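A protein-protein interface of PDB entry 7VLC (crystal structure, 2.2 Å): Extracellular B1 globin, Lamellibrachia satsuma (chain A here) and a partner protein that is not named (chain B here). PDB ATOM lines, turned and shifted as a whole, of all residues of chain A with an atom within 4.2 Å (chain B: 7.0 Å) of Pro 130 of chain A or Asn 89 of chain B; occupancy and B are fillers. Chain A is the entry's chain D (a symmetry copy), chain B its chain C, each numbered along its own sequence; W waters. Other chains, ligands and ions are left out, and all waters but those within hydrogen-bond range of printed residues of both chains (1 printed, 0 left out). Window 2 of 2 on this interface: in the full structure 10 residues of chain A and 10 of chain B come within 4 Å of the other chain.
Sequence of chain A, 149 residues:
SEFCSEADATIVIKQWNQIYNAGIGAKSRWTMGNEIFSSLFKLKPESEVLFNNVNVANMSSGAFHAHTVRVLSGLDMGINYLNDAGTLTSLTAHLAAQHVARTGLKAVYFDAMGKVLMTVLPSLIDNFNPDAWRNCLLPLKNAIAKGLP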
ATOM      1  N   PHE A 128     -30.656  13.881 -25.443  1.00  0.00           N
ATOM      2  CA  PHE A 128     -29.966  14.164 -24.192  1.00  0.00           C
ATOM      3  C   PHE A 128     -30.040  15.650 -23.878  1.00  0.00           C
ATOM      4  O   PHE A 128     -29.684  16.490 -24.709  1.00  0.00           O
ATOM      5  CB  PHE A 128     -28.508  13.713 -24.279  1.00  0.00           C
ATOM      6  CG  PHE A 128     -27.713  13.989 -23.038  1.00  0.00           C
ATOM      7  CD1 PHE A 128     -27.828  13.168 -21.925  1.00  0.00           C
ATOM      8  CD2 PHE A 128     -26.841  15.067 -22.983  1.00  0.00           C
ATOM      9  CE1 PHE A 128     -27.092  13.421 -20.781  1.00  0.00           C
ATOM     10  CE2 PHE A 128     -26.102  15.326 -21.845  1.00  0.00           C
ATOM     11  CZ  PHE A 128     -26.226  14.502 -20.742  1.00  0.00           C
ATOM     12  N   ASN A 129     -30.520  15.970 -22.675  1.00  0.00           N
ATOM     13  CA  ASN A 129     -30.698  17.349 -22.241  1.00  0.00           C
ATOM     14  C   ASN A 129     -29.536  17.746 -21.342  1.00  0.00           C
ATOM     15  O   ASN A 129     -29.583  17.490 -20.130  1.00  0.00           O
ATOM     16  CB  ASN A 129     -32.032  17.512 -21.509  1.00  0.00           C
ATOM     17  CG  ASN A 129     -32.394  18.968 -21.265  1.00  0.00           C
ATOM     18  OD1 ASN A 129     -31.539  19.789 -20.932  1.00  0.00           O
ATOM     19  ND2 ASN A 129     -33.670  19.291 -21.435  1.00  0.00           N
ATOM     20  N   PRO A 130     -28.495  18.400 -21.864  1.00  0.00           N
ATOM     21  CA  PRO A 130     -27.314  18.686 -21.032  1.00  0.00           C
ATOM     22  C   PRO A 130     -27.564  19.697 -19.925  1.00  0.00           C
ATOM     23  O   PRO A 130     -26.829  19.686 -18.928  1.00  0.00           O
ATOM     24  CB  PRO A 130     -26.294  19.216 -22.049  1.00  0.00           C
ATOM     25  CG  PRO A 130     -27.136  19.818 -23.132  1.00  0.00           C
ATOM     26  CD  PRO A 130     -28.357  18.942 -23.229  1.00  0.00           C
ATOM     27  N   ASP A 131     -28.563  20.571 -20.065  1.00  0.00           N
ATOM     28  CA  ASP A 131     -28.845  21.550 -19.019  1.00  0.00           C
ATOM     29  C   ASP A 131     -29.587  20.916 -17.850  1.00  0.00           C
ATOM     30  O   ASP A 131     -29.235  21.141 -16.688  1.00  0.00           O
ATOM     31  CB  ASP A 131     -29.648  22.721 -19.593  1.00  0.00           C
ATOM     32  CG  ASP A 131     -28.804  23.644 -20.449  1.00  0.00           C
ATOM     33  OD1 ASP A 131     -27.580  23.411 -20.563  1.00  0.00           O
ATOM     34  OD2 ASP A 131     -29.368  24.606 -21.009  1.00  0.00           O
ATOM     35  N   ALA A 132     -30.618  20.120 -18.136  1.00  0.00           N
ATOM     36  CA  ALA A 132     -31.306  19.404 -17.067  1.00  0.00           C
ATOM     37  C   ALA A 132     -30.352  18.467 -16.337  1.00  0.00           C
ATOM     38  O   ALA A 132     -30.437  18.307 -15.113  1.00  0.00           O
ATOM     39  CB  ALA A 132     -32.495  18.630 -17.637  1.00  0.00           C
ATOM     40  N   TRP A 133     -29.425  17.844 -17.071  1.00  0.00           N
ATOM     41  CA  TRP A 133     -28.454  16.961 -16.436  1.00  0.00           C
ATOM     42  C   TRP A 133     -27.444  17.750 -15.614  1.00  0.00           C
ATOM     43  O   TRP A 133     -27.091  17.340 -14.503  1.00  0.00           O
ATOM     44  CB  TRP A 133     -27.759  16.101 -17.492  1.00  0.00           C
ATOM     45  CG  TRP A 133     -28.549  14.874 -17.848  1.00  0.00           C
ATOM     46  CD1 TRP A 133     -29.548  14.774 -18.775  1.00  0.00           C
ATOM     47  CD2 TRP A 133     -28.412  13.570 -17.267  1.00  0.00           C
ATOM     48  NE1 TRP A 133     -30.039  13.488 -18.808  1.00  0.00           N
ATOM     49  CE2 TRP A 133     -29.357  12.730 -17.893  1.00  0.00           C
ATOM     50  CE3 TRP A 133     -27.580  13.032 -16.281  1.00  0.00           C
ATOM     51  CZ2 TRP A 133     -29.491  11.382 -17.563  1.00  0.00           C
ATOM     52  CZ3 TRP A 133     -27.714  11.694 -15.955  1.00  0.00           C
ATOM     53  CH2 TRP A 133     -28.663  10.883 -16.595  1.00  0.00           C
ATOM     54  N   ARG A 134     -26.972  18.888 -16.130  1.00  0.00           N
ATOM     55  CA  ARG A 134     -26.070  19.727 -15.345  1.00  0.00           C
ATOM     56  C   ARG A 134     -26.752  20.243 -14.087  1.00  0.00           C
ATOM     57  O   ARG A 134     -26.139  20.294 -13.016  1.00  0.00           O
ATOM     58  CB  ARG A 134     -25.558  20.901 -16.182  1.00  0.00           C
ATOM     59  CG  ARG A 134     -24.198  20.661 -16.803  1.00  0.00           C
ATOM     60  CD  ARG A 134     -23.724  21.855 -17.612  1.00  0.00           C
ATOM     61  NE  ARG A 134     -22.690  21.465 -18.567  1.00  0.00           N
ATOM     62  CZ  ARG A 134     -22.941  21.026 -19.796  1.00  0.00           C
ATOM     63  NH1 ARG A 134     -24.192  20.925 -20.219  1.00  0.00           N
ATOM     64  NH2 ARG A 134     -21.941  20.687 -20.602  1.00  0.00           N
ATOM     65  N   LEU B  81     -34.721  27.698 -28.304  1.00  0.00           N
ATOM     66  CA  LEU B  81     -33.806  26.571 -28.156  1.00  0.00           C
ATOM     67  C   LEU B  81     -33.529  26.209 -26.701  1.00  0.00           C
ATOM     68  O   LEU B  81     -32.807  25.240 -26.454  1.00  0.00           O
ATOM     69  CB  LEU B  81     -32.494  26.861 -28.888  1.00  0.00           C
ATOM     70  CG  LEU B  81     -32.575  26.790 -30.415  1.00  0.00           C
ATOM     71  CD1 LEU B  81     -31.260  27.218 -31.042  1.00  0.00           C
ATOM     72  CD2 LEU B  81     -32.963  25.383 -30.861  1.00  0.00           C
ATOM     73  N   ASP B  84     -34.297  22.745 -26.280  1.00  0.00           N
ATOM     74  CA  ASP B  84     -33.371  21.784 -26.880  1.00  0.00           C
ATOM     75  C   ASP B  84     -31.954  22.267 -26.601  1.00  0.00           C
ATOM     76  O   ASP B  84     -31.296  22.844 -27.479  1.00  0.00           O
ATOM     77  CB  ASP B  84     -33.629  21.630 -28.378  1.00  0.00           C
ATOM     78  CG  ASP B  84     -32.894  20.445 -28.978  1.00  0.00           C
ATOM     79  OD1 ASP B  84     -32.461  19.559 -28.212  1.00  0.00           O
ATOM     80  OD2 ASP B  84     -32.745  20.408 -30.217  1.00  0.00           O
ATOM     81  N   PRO B  85     -31.451  22.046 -25.385  1.00  0.00           N
ATOM     82  CA  PRO B  85     -30.165  22.649 -24.994  1.00  0.00           C
ATOM     83  C   PRO B  85     -28.971  22.153 -25.791  1.00  0.00           C
ATOM     84  O   PRO B  85     -27.965  22.872 -25.862  1.00  0.00           O
ATOM     85  CB  PRO B  85     -30.045  22.272 -23.510  1.00  0.00           C
ATOM     86  CG  PRO B  85     -31.450  22.055 -23.073  1.00  0.00           C
ATOM     87  CD  PRO B  85     -32.112  21.395 -24.243  1.00  0.00           C
ATOM     88  N   SER B  86     -29.038  20.955 -26.378  1.00  0.00           N
ATOM     89  CA  SER B  86     -27.961  20.491 -27.250  1.00  0.00           C
ATOM     90  C   SER B  86     -27.760  21.446 -28.418  1.00  0.00           C
ATOM     91  O   SER B  86     -26.652  21.951 -28.646  1.00  0.00           O
ATOM     92  CB  SER B  86     -28.270  19.085 -27.765  1.00  0.00           C
ATOM     93  OG  SER B  86     -28.385  18.168 -26.696  1.00  0.00           O
ATOM     94  N   THR B  87     -28.828  21.700 -29.176  1.00  0.00           N
ATOM     95  CA  THR B  87     -28.758  22.673 -30.260  1.00  0.00           C
ATOM     96  C   THR B  87     -28.490  24.077 -29.733  1.00  0.00           C
ATOM     97  O   THR B  87     -27.785  24.858 -30.382  1.00  0.00           O
ATOM     98  CB  THR B  87     -30.054  22.638 -31.064  1.00  0.00           C
ATOM     99  OG1 THR B  87     -30.320  21.281 -31.440  1.00  0.00           O
ATOM    100  CG2 THR B  87     -29.935  23.505 -32.323  1.00  0.00           C
ATOM    101  N   LEU B  88     -29.037  24.409 -28.563  1.00  0.00           N
ATOM    102  CA  LEU B  88     -28.799  25.723 -27.970  1.00  0.00           C
ATOM    103  C   LEU B  88     -27.308  25.971 -27.755  1.00  0.00           C
ATOM    104  O   LEU B  88     -26.789  27.044 -28.088  1.00  0.00           O
ATOM    105  CB  LEU B  88     -29.560  25.841 -26.649  1.00  0.00           C
ATOM    106  CG  LEU B  88     -29.280  27.071 -25.782  1.00  0.00           C
ATOM    107  CD1 LEU B  88     -29.857  28.333 -26.414  1.00  0.00           C
ATOM    108  CD2 LEU B  88     -29.824  26.867 -24.378  1.00  0.00           C
ATOM    109  N   ASN B  89     -26.601  24.975 -27.211  1.00  0.00           N
ATOM    110  CA  ASN B  89     -25.170  25.127 -26.960  1.00  0.00           C
ATOM    111  C   ASN B  89     -24.408  25.430 -28.247  1.00  0.00           C
ATOM    112  O   ASN B  89     -23.456  26.216 -28.239  1.00  0.00           O
ATOM    113  CB  ASN B  89     -24.620  23.872 -26.277  1.00  0.00           C
ATOM    114  CG  ASN B  89     -24.977  23.814 -24.801  1.00  0.00           C
ATOM    115  OD1 ASN B  89     -25.106  24.850 -24.149  1.00  0.00           O
ATOM    116  ND2 ASN B  89     -25.149  22.608 -24.271  1.00  0.00           N
ATOM    117  N   GLU B  90     -24.829  24.840 -29.367  1.00  0.00           N
ATOM    118  CA  GLU B  90     -24.186  25.141 -30.642  1.00  0.00           C
ATOM    119  C   GLU B  90     -24.517  26.554 -31.111  1.00  0.00           C
ATOM    120  O   GLU B  90     -23.652  27.256 -31.647  1.00  0.00           O
ATOM    121  CB  GLU B  90     -24.597  24.111 -31.693  1.00  0.00           C
ATOM    122  CG  GLU B  90     -24.061  22.714 -31.428  1.00  0.00           C
ATOM    123  CD  GLU B  90     -22.547  22.675 -31.419  1.00  0.00           C
ATOM    124  OE1 GLU B  90     -21.934  23.041 -32.446  1.00  0.00           O
ATOM    125  OE2 GLU B  90     -21.970  22.298 -30.376  1.00  0.00           O
ATOM    126  N   GLN B  91     -25.762  26.990 -30.917  1.00  0.00           N
ATOM    127  CA  GLN B  91     -26.149  28.325 -31.361  1.00  0.00           C
ATOM    128  C   GLN B  91     -25.489  29.403 -30.512  1.00  0.00           C
ATOM    129  O   GLN B  91     -25.100  30.457 -31.029  1.00  0.00           O
ATOM    130  CB  GLN B  91     -27.674  28.458 -31.336  1.00  0.00           C
ATOM    131  CG  GLN B  91     -28.207  29.852 -31.645  1.00  0.00           C
ATOM    132  CD  GLN B  91     -28.020  30.261 -33.096  1.00  0.00           C
ATOM    133  OE1 GLN B  91     -27.440  29.526 -33.898  1.00  0.00           O
ATOM    134  NE2 GLN B  91     -28.518  31.441 -33.441  1.00  0.00           N
ATOM    135  N   LEU B  92     -25.342  29.151 -29.210  1.00  0.00           N
ATOM    136  CA  LEU B  92     -24.704  30.128 -28.336  1.00  0.00           C
ATOM    137  C   LEU B  92     -23.211  30.245 -28.615  1.00  0.00           C
ATOM    138  O   LEU B  92     -22.616  31.300 -28.363  1.00  0.00           O
ATOM    139  CB  LEU B  92     -24.940  29.761 -26.872  1.00  0.00           C
ATOM    140  CG  LEU B  92     -26.392  29.770 -26.389  1.00  0.00           C
ATOM    141  CD1 LEU B  92     -26.458  29.529 -24.892  1.00  0.00           C
ATOM    142  CD2 LEU B  92     -27.086  31.073 -26.754  1.00  0.00           C
ATOM    143  N   SER B  93     -22.585  29.176 -29.121  1.00  0.00           N
ATOM    144  CA  SER B  93     -21.191  29.273 -29.539  1.00  0.00           C
ATOM    145  C   SER B  93     -21.056  30.129 -30.789  1.00  0.00           C
ATOM    146  O   SER B  93     -20.136  30.948 -30.889  1.00  0.00           O
ATOM    147  CB  SER B  93     -20.607  27.882 -29.783  1.00  0.00           C
ATOM    148  OG  SER B  93     -20.610  27.116 -28.593  1.00  0.00           O
ATOM    149  N   HIS B  94     -21.966  29.953 -31.750  1.00  0.00           N
ATOM    150  CA  HIS B  94     -21.927  30.758 -32.965  1.00  0.00           C
ATOM    151  C   HIS B  94     -22.134  32.232 -32.649  1.00  0.00           C
ATOM    152  O   HIS B  94     -21.507  33.102 -33.266  1.00  0.00           O
ATOM    153  CB  HIS B  94     -22.984  30.267 -33.950  1.00  0.00           C
ATOM    154  CG  HIS B  94     -22.941  30.953 -35.279  1.00  0.00           C
ATOM    155  ND1 HIS B  94     -22.172  30.495 -36.327  1.00  0.00           N
ATOM    156  CD2 HIS B  94     -23.574  32.061 -35.734  1.00  0.00           C
ATOM    157  CE1 HIS B  94     -22.338  31.288 -37.371  1.00  0.00           C
ATOM    158  NE2 HIS B  94     -23.182  32.247 -37.037  1.00  0.00           N
ATOM    159  N   ARG B 139     -28.317  32.411 -18.266  1.00  0.00           N
ATOM    160  CA  ARG B 139     -27.920  31.148 -18.882  1.00  0.00           C
ATOM    161  C   ARG B 139     -27.609  31.337 -20.361  1.00  0.00           C
ATOM    162  O   ARG B 139     -26.662  30.737 -20.887  1.00  0.00           O
ATOM    163  CB  ARG B 139     -29.025  30.109 -18.689  1.00  0.00           C
ATOM    164  CG  ARG B 139     -29.005  28.963 -19.691  1.00  0.00           C
ATOM    165  CD  ARG B 139     -27.826  28.040 -19.462  1.00  0.00           C
ATOM    166  NE  ARG B 139     -27.783  26.954 -20.438  1.00  0.00           N
ATOM    167  CZ  ARG B 139     -27.046  26.968 -21.543  1.00  0.00           C
ATOM    168  NH1 ARG B 139     -26.281  28.016 -21.821  1.00  0.00           N
ATOM    169  NH2 ARG B 139     -27.069  25.930 -22.367  1.00  0.00           N
ATOM    170  N   GLY B 143     -23.343  31.441 -22.372  1.00  0.00           N
ATOM    171  CA  GLY B 143     -22.806  30.851 -23.586  1.00  0.00           C
ATOM    172  C   GLY B 143     -22.338  31.856 -24.616  1.00  0.00           C
ATOM    173  O   GLY B 143     -21.495  31.522 -25.453  1.00  0.00           O
HETATM  174  O   HOH W   1     -31.029  18.866 -26.039  1.00  0.00           O
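The side-chain hydroxyl of Ser 86 of chain B lies within hydrogen-bond range of the backbone carbonyl oxygen of Phe 128 of chain A (2.9 Å). The side-chain carboxylate (OD2) of Asp 131 of chain A lies within salt-bridge range of the guanidinium group (NE) of Arg 139 of chain B (2.9 Å).
The side-chain amide nitrogen (ND2) of Asn 89 of chain B lies within hydrogen-bond range of the backbone carbonyl oxygen (O) of Pro 85 of chain B (3.2 Å). OG of Ser 93 of chain B sits at hydrogen-bond distance from O of Asn 89 of chain B (3.0 Å). The side-chain amide oxygen (OD1) of Asn 89 of chain B is in hydrogen-bond range of the guanidinium group (NH2) of Arg 139 of chain B (2.9 Å). The side-chain amide oxygen of Asn 129 of chain A is in hydrogen-bond range of the backbone NH of Asp 131 of chain A (3.2 Å). The side-chain amide oxygen of Asn 129 of chain A sits at hydrogen-bond distance from the backbone NH of Ala 132 of chain A (3.0 Å). The guanidinium group of Arg 134 of chain A lies within hydrogen-bond range of the backbone carbonyl oxygen of Pro 130 of chain A, at 3.2 Å.
Pro 85 of chain B touches Asn 129 of chain A. CD of Pro 130 of chain A touches CB of Pro 85 of chain B (3.7 Å). CD of Pro 130 of chain A touches OG of Ser 86 of chain B, 3.6 Å away. Asn 89 of chain B touches Pro 130 of chain A (ND2 to CG, 3.6 Å). Asp 131 of chain A touches Pro 85 of chain B (OD2 to CB, 3.5 Å).
Of chain B, only Pro 85, Ser 86 and Asn 89 come within 4 Å of Pro 130 of chain A. Of chain A, only Pro 130 comes within 4 Å of Asn 89 of chain B. Printed residues of chain A within 4 Å of Ser 86 of chain B: Phe 128 and Pro 130. Printed residues of chain A within 4 Å of Arg 139 of chain B: Asp 131. The nearest residue of chain B that does not touch Pro 130 of chain A is Asp 84 of chain B (5.9 Å). The nearest printed residue of chain A that does not touch Arg 139 of chain B is Arg 134 of chain A (6.2 Å).
Hydrophobic or aromatic side chains of chain A that line the printed part of chain B: Pro 130. Printed residues of chain B that touch a printed residue of chain A: Pro 85, Ser 86, Asn 89 and Arg 139. Hydrophobic or aromatic side chains of chain B that line the printed part of chain A: Pro 85. Among the printed residues, 7 pairs touch across the chains. Among the printed residues, Asp or Glu carboxylates within 4 Å of a Lys or Arg side-chain nitrogen of the other chain: Asp 131 of chain A with Arg 139 of chain B.
Water W1 lies within hydrogen-bond range of OD1 of Asp 84 of chain B (2.7 Å), OG of Ser 86 of chain B (2.8 Å) and O of Phe 128 of chain A (3.0 Å).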
